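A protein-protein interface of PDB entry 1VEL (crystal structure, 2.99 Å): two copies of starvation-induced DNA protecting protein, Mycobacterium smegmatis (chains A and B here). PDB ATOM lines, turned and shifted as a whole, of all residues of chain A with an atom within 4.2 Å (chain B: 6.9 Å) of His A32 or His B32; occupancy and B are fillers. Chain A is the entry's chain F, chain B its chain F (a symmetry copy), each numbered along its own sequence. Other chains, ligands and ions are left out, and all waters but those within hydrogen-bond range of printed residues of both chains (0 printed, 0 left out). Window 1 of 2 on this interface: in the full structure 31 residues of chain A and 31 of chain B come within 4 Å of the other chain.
A ring nitrogen (NE2) of His A32 lies within hydrogen-bond range of the side-chain amide oxygen (OD1) of Asn A29. The side-chain carboxylate (OE2) of Glu B59 lies within salt-bridge range of the guanidinium group (NH1) of Arg B62 (3.5 Å). NE2 of His B32 sits at hydrogen-bond distance from OD1 of Asn B29, at 2.9 Å.
Among the printed residues, merely in contact across the chains: His A32 with His B32 (3.98 Å), Leu A33 with Gly B81 (3.6 Å) and Arg A62 with Arg B62 (3.5 Å).
His A32 touches just one residue of chain B: His B32 (3.98 Å). Of chain A, only His A32 (3.98 Å) comes within 4 Å of His B32. Printed residues of chain B within 4 Å of Arg A62: Arg B62 (3.5 Å). Printed residues of chain A within 4 Å of Arg B62: Arg A62. The nearest residue of chain B that does not touch His A32 is Leu B33 (4.1 Å).
Hydrophobic or aromatic side chains of chain A that line the printed part of chain B: His A32 and Leu A33. Of the 21 printed residues of chain B, 3 touch a printed residue of chain A. Among the printed residues, 3 pairs touch across the chains. Among the printed residues, no Asp or Glu carboxylate lies within 4 Å of a Lys or Arg side-chain nitrogen of the other chain.
His A32 touches its own counterpart, His B32. Arg B62 touches its own counterpart, Arg A62. Of the 3 pairs that touch across the chains among the printed residues, 2 have their exchanged pair printed and touching as well.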
ATOM      1  N   TYR A  28      18.723  -1.691 -13.484  1.00  0.00           N
ATOM      2  CA  TYR A  28      18.129  -1.225 -12.239  1.00  0.00           C
ATOM      3  C   TYR A  28      17.420  -2.355 -11.493  1.00  0.00           C
ATOM      4  O   TYR A  28      17.627  -2.542 -10.290  1.00  0.00           O
ATOM      5  CB  TYR A  28      17.139  -0.103 -12.529  1.00  0.00           C
ATOM      6  CG  TYR A  28      17.778   1.232 -12.853  1.00  0.00           C
ATOM      7  CD1 TYR A  28      17.029   2.254 -13.450  1.00  0.00           C
ATOM      8  CD2 TYR A  28      19.108   1.494 -12.527  1.00  0.00           C
ATOM      9  CE1 TYR A  28      17.584   3.500 -13.714  1.00  0.00           C
ATOM     10  CE2 TYR A  28      19.681   2.743 -12.787  1.00  0.00           C
ATOM     11  CZ  TYR A  28      18.909   3.742 -13.380  1.00  0.00           C
ATOM     12  OH  TYR A  28      19.440   4.985 -13.642  1.00  0.00           O
ATOM     13  N   ASN A  29      16.575  -3.096 -12.205  1.00  0.00           N
ATOM     14  CA  ASN A  29      15.853  -4.203 -11.598  1.00  0.00           C
ATOM     15  C   ASN A  29      16.812  -5.232 -11.019  1.00  0.00           C
ATOM     16  O   ASN A  29      16.631  -5.697  -9.895  1.00  0.00           O
ATOM     17  CB  ASN A  29      14.924  -4.873 -12.611  1.00  0.00           C
ATOM     18  CG  ASN A  29      13.626  -4.111 -12.798  1.00  0.00           C
ATOM     19  OD1 ASN A  29      13.064  -3.577 -11.835  1.00  0.00           O
ATOM     20  ND2 ASN A  29      13.133  -4.069 -14.035  1.00  0.00           N
ATOM     21  N   ASP A  30      17.840  -5.592 -11.775  1.00  0.00           N
ATOM     22  CA  ASP A  30      18.797  -6.563 -11.269  1.00  0.00           C
ATOM     23  C   ASP A  30      19.438  -6.015  -9.992  1.00  0.00           C
ATOM     24  O   ASP A  30      19.674  -6.756  -9.036  1.00  0.00           O
ATOM     25  CB  ASP A  30      19.877  -6.846 -12.318  1.00  0.00           C
ATOM     26  CG  ASP A  30      20.875  -7.888 -11.861  1.00  0.00           C
ATOM     27  OD1 ASP A  30      20.975  -8.941 -12.516  1.00  0.00           O
ATOM     28  OD2 ASP A  30      21.559  -7.659 -10.846  1.00  0.00           O
ATOM     29  N   LEU A  31      19.693  -4.708  -9.975  1.00  0.00           N
ATOM     30  CA  LEU A  31      20.324  -4.068  -8.829  1.00  0.00           C
ATOM     31  C   LEU A  31      19.453  -4.066  -7.579  1.00  0.00           C
ATOM     32  O   LEU A  31      19.913  -4.475  -6.514  1.00  0.00           O
ATOM     33  CB  LEU A  31      20.729  -2.625  -9.168  1.00  0.00           C
ATOM     34  CG  LEU A  31      22.111  -2.129  -8.698  1.00  0.00           C
ATOM     35  CD1 LEU A  31      22.157  -0.621  -8.738  1.00  0.00           C
ATOM     36  CD2 LEU A  31      22.396  -2.587  -7.283  1.00  0.00           C
ATOM     37  N   HIS A  32      18.202  -3.615  -7.700  1.00  0.00           N
ATOM     38  CA  HIS A  32      17.317  -3.551  -6.537  1.00  0.00           C
ATOM     39  C   HIS A  32      16.813  -4.907  -6.051  1.00  0.00           C
ATOM     40  O   HIS A  32      15.941  -4.989  -5.191  1.00  0.00           O
ATOM     41  CB  HIS A  32      16.153  -2.567  -6.789  1.00  0.00           C
ATOM     42  CG  HIS A  32      14.995  -3.141  -7.546  1.00  0.00           C
ATOM     43  ND1 HIS A  32      14.190  -4.139  -7.037  1.00  0.00           N
ATOM     44  CD2 HIS A  32      14.486  -2.831  -8.763  1.00  0.00           C
ATOM     45  CE1 HIS A  32      13.238  -4.420  -7.911  1.00  0.00           C
ATOM     46  NE2 HIS A  32      13.396  -3.640  -8.967  1.00  0.00           N
ATOM     47  N   LEU A  33      17.363  -5.971  -6.615  1.00  0.00           N
ATOM     48  CA  LEU A  33      17.017  -7.312  -6.185  1.00  0.00           C
ATOM     49  C   LEU A  33      18.291  -7.735  -5.486  1.00  0.00           C
ATOM     50  O   LEU A  33      18.276  -8.156  -4.336  1.00  0.00           O
ATOM     51  CB  LEU A  33      16.741  -8.245  -7.368  1.00  0.00           C
ATOM     52  CG  LEU A  33      15.444  -8.117  -8.177  1.00  0.00           C
ATOM     53  CD1 LEU A  33      15.470  -9.122  -9.308  1.00  0.00           C
ATOM     54  CD2 LEU A  33      14.239  -8.382  -7.313  1.00  0.00           C
ATOM     55  N   THR A  34      19.405  -7.588  -6.192  1.00  0.00           N
ATOM     56  CA  THR A  34      20.706  -7.938  -5.646  1.00  0.00           C
ATOM     57  C   THR A  34      20.957  -7.199  -4.331  1.00  0.00           C
ATOM     58  O   THR A  34      21.427  -7.787  -3.357  1.00  0.00           O
ATOM     59  CB  THR A  34      21.833  -7.588  -6.643  1.00  0.00           C
ATOM     60  OG1 THR A  34      21.684  -8.382  -7.827  1.00  0.00           O
ATOM     61  CG2 THR A  34      23.194  -7.870  -6.033  1.00  0.00           C
ATOM     62  N   LYS A  36      18.837  -6.056  -2.060  1.00  0.00           N
ATOM     63  CA  LYS A  36      18.075  -6.685  -0.975  1.00  0.00           C
ATOM     64  C   LYS A  36      18.683  -8.039  -0.637  1.00  0.00           C
ATOM     65  O   LYS A  36      18.660  -8.465   0.511  1.00  0.00           O
ATOM     66  CB  LYS A  36      16.606  -6.891  -1.362  1.00  0.00           C
ATOM     67  CG  LYS A  36      15.782  -5.619  -1.514  1.00  0.00           C
ATOM     68  CD  LYS A  36      14.783  -5.411  -0.371  1.00  0.00           C
ATOM     69  CE  LYS A  36      15.463  -4.938   0.902  1.00  0.00           C
ATOM     70  NZ  LYS A  36      14.511  -4.668   2.038  1.00  0.00           N
ATOM     71  N   VAL A  58      18.035   0.670  -2.033  1.00  0.00           N
ATOM     72  CA  VAL A  58      17.116  -0.253  -2.668  1.00  0.00           C
ATOM     73  C   VAL A  58      15.869   0.503  -3.082  1.00  0.00           C
ATOM     74  O   VAL A  58      15.375   0.340  -4.189  1.00  0.00           O
ATOM     75  CB  VAL A  58      16.694  -1.379  -1.709  1.00  0.00           C
ATOM     76  CG1 VAL A  58      15.567  -2.182  -2.328  1.00  0.00           C
ATOM     77  CG2 VAL A  58      17.880  -2.284  -1.403  1.00  0.00           C
ATOM     78  N   VAL A  61      16.782   3.063  -6.132  1.00  0.00           N
ATOM     79  CA  VAL A  61      16.927   2.342  -7.391  1.00  0.00           C
ATOM     80  C   VAL A  61      15.586   1.811  -7.873  1.00  0.00           C
ATOM     81  O   VAL A  61      15.300   1.858  -9.062  1.00  0.00           O
ATOM     82  CB  VAL A  61      17.927   1.158  -7.264  1.00  0.00           C
ATOM     83  CG1 VAL A  61      18.109   0.461  -8.621  1.00  0.00           C
ATOM     84  CG2 VAL A  61      19.266   1.669  -6.773  1.00  0.00           C
ATOM     85  N   ARG A  62      14.768   1.306  -6.954  1.00  0.00           N
ATOM     86  CA  ARG A  62      13.446   0.780  -7.305  1.00  0.00           C
ATOM     87  C   ARG A  62      12.609   1.878  -7.945  1.00  0.00           C
ATOM     88  O   ARG A  62      11.777   1.626  -8.828  1.00  0.00           O
ATOM     89  CB  ARG A  62      12.708   0.283  -6.062  1.00  0.00           C
ATOM     90  CG  ARG A  62      12.756  -1.204  -5.816  1.00  0.00           C
ATOM     91  CD  ARG A  62      12.125  -1.506  -4.475  1.00  0.00           C
ATOM     92  NE  ARG A  62      12.314  -2.886  -4.049  1.00  0.00           N
ATOM     93  CZ  ARG A  62      12.000  -3.326  -2.838  1.00  0.00           C
ATOM     94  NH1 ARG A  62      11.490  -2.487  -1.955  1.00  0.00           N
ATOM     95  NH2 ARG A  62      12.192  -4.596  -2.514  1.00  0.00           N
ATOM     96  N   LEU B  25       9.424 -16.989  -1.567  1.00  0.00           N
ATOM     97  CA  LEU B  25      10.212 -15.779  -1.777  1.00  0.00           C
ATOM     98  C   LEU B  25      10.302 -15.440  -3.257  1.00  0.00           C
ATOM     99  O   LEU B  25       9.987 -14.320  -3.663  1.00  0.00           O
ATOM    100  CB  LEU B  25      11.625 -15.949  -1.216  1.00  0.00           C
ATOM    101  CG  LEU B  25      12.393 -14.672  -0.843  1.00  0.00           C
ATOM    102  CD1 LEU B  25      13.881 -14.966  -0.899  1.00  0.00           C
ATOM    103  CD2 LEU B  25      12.067 -13.533  -1.785  1.00  0.00           C
ATOM    104  N   THR B  27       8.446 -16.458  -5.527  1.00  0.00           N
ATOM    105  CA  THR B  27       7.094 -16.190  -5.999  1.00  0.00           C
ATOM    106  C   THR B  27       6.803 -14.703  -5.803  1.00  0.00           C
ATOM    107  O   THR B  27       6.351 -14.017  -6.723  1.00  0.00           O
ATOM    108  CB  THR B  27       6.043 -17.011  -5.222  1.00  0.00           C
ATOM    109  OG1 THR B  27       6.173 -18.402  -5.550  1.00  0.00           O
ATOM    110  CG2 THR B  27       4.641 -16.542  -5.573  1.00  0.00           C
ATOM    111  N   TYR B  28       7.070 -14.211  -4.598  1.00  0.00           N
ATOM    112  CA  TYR B  28       6.851 -12.807  -4.277  1.00  0.00           C
ATOM    113  C   TYR B  28       7.650 -11.884  -5.196  1.00  0.00           C
ATOM    114  O   TYR B  28       7.107 -10.924  -5.751  1.00  0.00           O
ATOM    115  CB  TYR B  28       7.240 -12.546  -2.826  1.00  0.00           C
ATOM    116  CG  TYR B  28       6.241 -13.051  -1.806  1.00  0.00           C
ATOM    117  CD1 TYR B  28       6.600 -13.178  -0.458  1.00  0.00           C
ATOM    118  CD2 TYR B  28       4.930 -13.359  -2.170  1.00  0.00           C
ATOM    119  CE1 TYR B  28       5.685 -13.596   0.500  1.00  0.00           C
ATOM    120  CE2 TYR B  28       3.997 -13.781  -1.217  1.00  0.00           C
ATOM    121  CZ  TYR B  28       4.385 -13.895   0.119  1.00  0.00           C
ATOM    122  OH  TYR B  28       3.489 -14.301   1.082  1.00  0.00           O
ATOM    123  N   ASN B  29       8.942 -12.169  -5.344  1.00  0.00           N
ATOM    124  CA  ASN B  29       9.794 -11.363  -6.203  1.00  0.00           C
ATOM    125  C   ASN B  29       9.276 -11.348  -7.633  1.00  0.00           C
ATOM    126  O   ASN B  29       9.202 -10.295  -8.264  1.00  0.00           O
ATOM    127  CB  ASN B  29      11.236 -11.872  -6.179  1.00  0.00           C
ATOM    128  CG  ASN B  29      11.996 -11.398  -4.956  1.00  0.00           C
ATOM    129  OD1 ASN B  29      11.830 -10.256  -4.513  1.00  0.00           O
ATOM    130  ND2 ASN B  29      12.848 -12.265  -4.411  1.00  0.00           N
ATOM    131  N   ASP B  30       8.910 -12.511  -8.155  1.00  0.00           N
ATOM    132  CA  ASP B  30       8.396 -12.558  -9.514  1.00  0.00           C
ATOM    133  C   ASP B  30       7.139 -11.689  -9.603  1.00  0.00           C
ATOM    134  O   ASP B  30       6.922 -10.993 -10.596  1.00  0.00           O
ATOM    135  CB  ASP B  30       8.066 -14.000  -9.912  1.00  0.00           C
ATOM    136  CG  ASP B  30       7.570 -14.112 -11.338  1.00  0.00           C
ATOM    137  OD1 ASP B  30       8.226 -14.798 -12.142  1.00  0.00           O
ATOM    138  OD2 ASP B  30       6.526 -13.514 -11.658  1.00  0.00           O
ATOM    139  N   LEU B  31       6.328 -11.717  -8.547  1.00  0.00           N
ATOM    140  CA  LEU B  31       5.087 -10.955  -8.518  1.00  0.00           C
ATOM    141  C   LEU B  31       5.302  -9.447  -8.500  1.00  0.00           C
ATOM    142  O   LEU B  31       4.711  -8.737  -9.314  1.00  0.00           O
ATOM    143  CB  LEU B  31       4.230 -11.360  -7.307  1.00  0.00           C
ATOM    144  CG  LEU B  31       2.715 -11.550  -7.521  1.00  0.00           C
ATOM    145  CD1 LEU B  31       2.002 -11.521  -6.191  1.00  0.00           C
ATOM    146  CD2 LEU B  31       2.153 -10.452  -8.400  1.00  0.00           C
ATOM    147  N   HIS B  32       6.142  -8.953  -7.587  1.00  0.00           N
ATOM    148  CA  HIS B  32       6.372  -7.513  -7.488  1.00  0.00           C
ATOM    149  C   HIS B  32       7.211  -6.927  -8.620  1.00  0.00           C
ATOM    150  O   HIS B  32       7.616  -5.769  -8.578  1.00  0.00           O
ATOM    151  CB  HIS B  32       6.949  -7.145  -6.102  1.00  0.00           C
ATOM    152  CG  HIS B  32       8.431  -7.317  -5.970  1.00  0.00           C
ATOM    153  ND1 HIS B  32       9.338  -6.552  -6.676  1.00  0.00           N
ATOM    154  CD2 HIS B  32       9.165  -8.144  -5.187  1.00  0.00           C
ATOM    155  CE1 HIS B  32      10.565  -6.905  -6.333  1.00  0.00           C
ATOM    156  NE2 HIS B  32      10.487  -7.870  -5.433  1.00  0.00           N
ATOM    157  N   LEU B  33       7.478  -7.740  -9.631  1.00  0.00           N
ATOM    158  CA  LEU B  33       8.205  -7.275 -10.796  1.00  0.00           C
ATOM    159  C   LEU B  33       7.111  -7.266 -11.842  1.00  0.00           C
ATOM    160  O   LEU B  33       6.873  -6.263 -12.503  1.00  0.00           O
ATOM    161  CB  LEU B  33       9.311  -8.251 -11.213  1.00  0.00           C
ATOM    162  CG  LEU B  33      10.601  -8.365 -10.392  1.00  0.00           C
ATOM    163  CD1 LEU B  33      11.478  -9.436 -11.004  1.00  0.00           C
ATOM    164  CD2 LEU B  33      11.355  -7.060 -10.384  1.00  0.00           C
ATOM    165  N   THR B  34       6.423  -8.395 -11.959  1.00  0.00           N
ATOM    166  CA  THR B  34       5.333  -8.529 -12.911  1.00  0.00           C
ATOM    167  C   THR B  34       4.285  -7.437 -12.691  1.00  0.00           C
ATOM    168  O   THR B  34       3.805  -6.823 -13.642  1.00  0.00           O
ATOM    169  CB  THR B  34       4.655  -9.911 -12.780  1.00  0.00           C
ATOM    170  OG1 THR B  34       5.595 -10.936 -13.122  1.00  0.00           O
ATOM    171  CG2 THR B  34       3.460 -10.012 -13.710  1.00  0.00           C
ATOM    172  N   LEU B  35       3.932  -7.196 -11.434  1.00  0.00           N
ATOM    173  CA  LEU B  35       2.946  -6.177 -11.115  1.00  0.00           C
ATOM    174  C   LEU B  35       3.350  -4.828 -11.707  1.00  0.00           C
ATOM    175  O   LEU B  35       2.556  -4.202 -12.404  1.00  0.00           O
ATOM    176  CB  LEU B  35       2.778  -6.077  -9.599  1.00  0.00           C
ATOM    177  CG  LEU B  35       1.418  -6.436  -8.994  1.00  0.00           C
ATOM    178  CD1 LEU B  35       0.661  -7.420  -9.881  1.00  0.00           C
ATOM    179  CD2 LEU B  35       1.653  -7.006  -7.595  1.00  0.00           C
ATOM    180  N   LYS B  36       4.581  -4.385 -11.443  1.00  0.00           N
ATOM    181  CA  LYS B  36       5.062  -3.108 -11.985  1.00  0.00           C
ATOM    182  C   LYS B  36       5.068  -3.165 -13.506  1.00  0.00           C
ATOM    183  O   LYS B  36       4.839  -2.162 -14.169  1.00  0.00           O
ATOM    184  CB  LYS B  36       6.482  -2.789 -11.502  1.00  0.00           C
ATOM    185  CG  LYS B  36       6.614  -2.472 -10.018  1.00  0.00           C
ATOM    186  CD  LYS B  36       6.878  -0.988  -9.741  1.00  0.00           C
ATOM    187  CE  LYS B  36       5.626  -0.145  -9.911  1.00  0.00           C
ATOM    188  NZ  LYS B  36       5.826   1.314  -9.596  1.00  0.00           N
ATOM    189  N   HIS B  37       5.336  -4.348 -14.050  1.00  0.00           N
ATOM    190  CA  HIS B  37       5.365  -4.540 -15.493  1.00  0.00           C
ATOM    191  C   HIS B  37       4.014  -4.204 -16.112  1.00  0.00           C
ATOM    192  O   HIS B  37       3.955  -3.503 -17.118  1.00  0.00           O
ATOM    193  CB  HIS B  37       5.727  -5.983 -15.839  1.00  0.00           C
ATOM    194  CG  HIS B  37       5.680  -6.280 -17.304  1.00  0.00           C
ATOM    195  ND1 HIS B  37       6.761  -6.088 -18.137  1.00  0.00           N
ATOM    196  CD2 HIS B  37       4.668  -6.715 -18.092  1.00  0.00           C
ATOM    197  CE1 HIS B  37       6.414  -6.392 -19.376  1.00  0.00           C
ATOM    198  NE2 HIS B  37       5.150  -6.775 -19.376  1.00  0.00           N
ATOM    199  N   GLN B  57      -0.099  -2.517  -3.956  1.00  0.00           N
ATOM    200  CA  GLN B  57       0.080  -3.970  -3.939  1.00  0.00           C
ATOM    201  C   GLN B  57       1.556  -4.268  -4.178  1.00  0.00           C
ATOM    202  O   GLN B  57       2.173  -5.076  -3.485  1.00  0.00           O
ATOM    203  CB  GLN B  57      -0.765  -4.598  -5.057  1.00  0.00           C
ATOM    204  CG  GLN B  57      -0.714  -6.119  -5.174  1.00  0.00           C
ATOM    205  CD  GLN B  57      -1.234  -6.821  -3.942  1.00  0.00           C
ATOM    206  OE1 GLN B  57      -2.169  -6.355  -3.297  1.00  0.00           O
ATOM    207  NE2 GLN B  57      -0.642  -7.956  -3.616  1.00  0.00           N
ATOM    208  N   VAL B  58       2.122  -3.610  -5.179  1.00  0.00           N
ATOM    209  CA  VAL B  58       3.527  -3.804  -5.480  1.00  0.00           C
ATOM    210  C   VAL B  58       4.337  -3.554  -4.223  1.00  0.00           C
ATOM    211  O   VAL B  58       5.234  -4.318  -3.893  1.00  0.00           O
ATOM    212  CB  VAL B  58       4.012  -2.823  -6.561  1.00  0.00           C
ATOM    213  CG1 VAL B  58       5.522  -2.900  -6.680  1.00  0.00           C
ATOM    214  CG2 VAL B  58       3.361  -3.149  -7.899  1.00  0.00           C
ATOM    215  N   GLU B  59       4.002  -2.484  -3.515  1.00  0.00           N
ATOM    216  CA  GLU B  59       4.736  -2.132  -2.313  1.00  0.00           C
ATOM    217  C   GLU B  59       4.513  -3.138  -1.189  1.00  0.00           C
ATOM    218  O   GLU B  59       5.421  -3.408  -0.408  1.00  0.00           O
ATOM    219  CB  GLU B  59       4.363  -0.717  -1.855  1.00  0.00           C
ATOM    220  CG  GLU B  59       5.553   0.101  -1.318  1.00  0.00           C
ATOM    221  CD  GLU B  59       6.619   0.397  -2.382  1.00  0.00           C
ATOM    222  OE1 GLU B  59       6.256   0.967  -3.433  1.00  0.00           O
ATOM    223  OE2 GLU B  59       7.813   0.074  -2.169  1.00  0.00           O
ATOM    224  N   LEU B  60       3.311  -3.703  -1.119  1.00  0.00           N
ATOM    225  CA  LEU B  60       2.971  -4.687  -0.094  1.00  0.00           C
ATOM    226  C   LEU B  60       3.773  -5.956  -0.336  1.00  0.00           C
ATOM    227  O   LEU B  60       4.518  -6.405   0.531  1.00  0.00           O
ATOM    228  CB  LEU B  60       1.489  -5.027  -0.174  1.00  0.00           C
ATOM    229  CG  LEU B  60       0.705  -5.327   1.096  1.00  0.00           C
ATOM    230  CD1 LEU B  60       0.164  -4.033   1.674  1.00  0.00           C
ATOM    231  CD2 LEU B  60      -0.453  -6.243   0.757  1.00  0.00           C
ATOM    232  N   VAL B  61       3.605  -6.532  -1.523  1.00  0.00           N
ATOM    233  CA  VAL B  61       4.306  -7.756  -1.895  1.00  0.00           C
ATOM    234  C   VAL B  61       5.809  -7.597  -1.725  1.00  0.00           C
ATOM    235  O   VAL B  61       6.475  -8.517  -1.268  1.00  0.00           O
ATOM    236  CB  VAL B  61       4.000  -8.170  -3.362  1.00  0.00           C
ATOM    237  CG1 VAL B  61       4.698  -9.496  -3.702  1.00  0.00           C
ATOM    238  CG2 VAL B  61       2.505  -8.321  -3.552  1.00  0.00           C
ATOM    239  N   ARG B  62       6.341  -6.435  -2.093  1.00  0.00           N
ATOM    240  CA  ARG B  62       7.776  -6.168  -1.960  1.00  0.00           C
ATOM    241  C   ARG B  62       8.187  -6.289  -0.500  1.00  0.00           C
ATOM    242  O   ARG B  62       9.309  -6.704  -0.177  1.00  0.00           O
ATOM    243  CB  ARG B  62       8.116  -4.756  -2.435  1.00  0.00           C
ATOM    244  CG  ARG B  62       8.666  -4.644  -3.834  1.00  0.00           C
ATOM    245  CD  ARG B  62       8.793  -3.183  -4.203  1.00  0.00           C
ATOM    246  NE  ARG B  62       9.111  -2.970  -5.608  1.00  0.00           N
ATOM    247  CZ  ARG B  62       9.098  -1.778  -6.188  1.00  0.00           C
ATOM    248  NH1 ARG B  62       8.781  -0.713  -5.474  1.00  0.00           N
ATOM    249  NH2 ARG B  62       9.403  -1.651  -7.471  1.00  0.00           N
ATOM    250  N   GLY B  63       7.268  -5.906   0.378  1.00  0.00           N
ATOM    251  CA  GLY B  63       7.534  -5.968   1.799  1.00  0.00           C
ATOM    252  C   GLY B  63       7.513  -7.411   2.232  1.00  0.00           C
ATOM    253  O   GLY B  63       8.295  -7.849   3.080  1.00  0.00           O
ATOM    254  N   ALA B  65       8.306  -9.868   0.354  1.00  0.00           N
ATOM    255  CA  ALA B  65       9.542 -10.449  -0.155  1.00  0.00           C
ATOM    256  C   ALA B  65      10.511 -10.531   1.003  1.00  0.00           C
ATOM    257  O   ALA B  65      11.065 -11.599   1.307  1.00  0.00           O
ATOM    258  CB  ALA B  65      10.133  -9.560  -1.233  1.00  0.00           C
ATOM    259  N   GLY B  81      17.865 -14.178  -3.349  1.00  0.00           N
ATOM    260  CA  GLY B  81      16.983 -13.184  -3.929  1.00  0.00           C
ATOM    261  C   GLY B  81      17.460 -12.486  -5.182  1.00  0.00           C
ATOM    262  O   GLY B  81      17.064 -11.347  -5.435  1.00  0.00           O
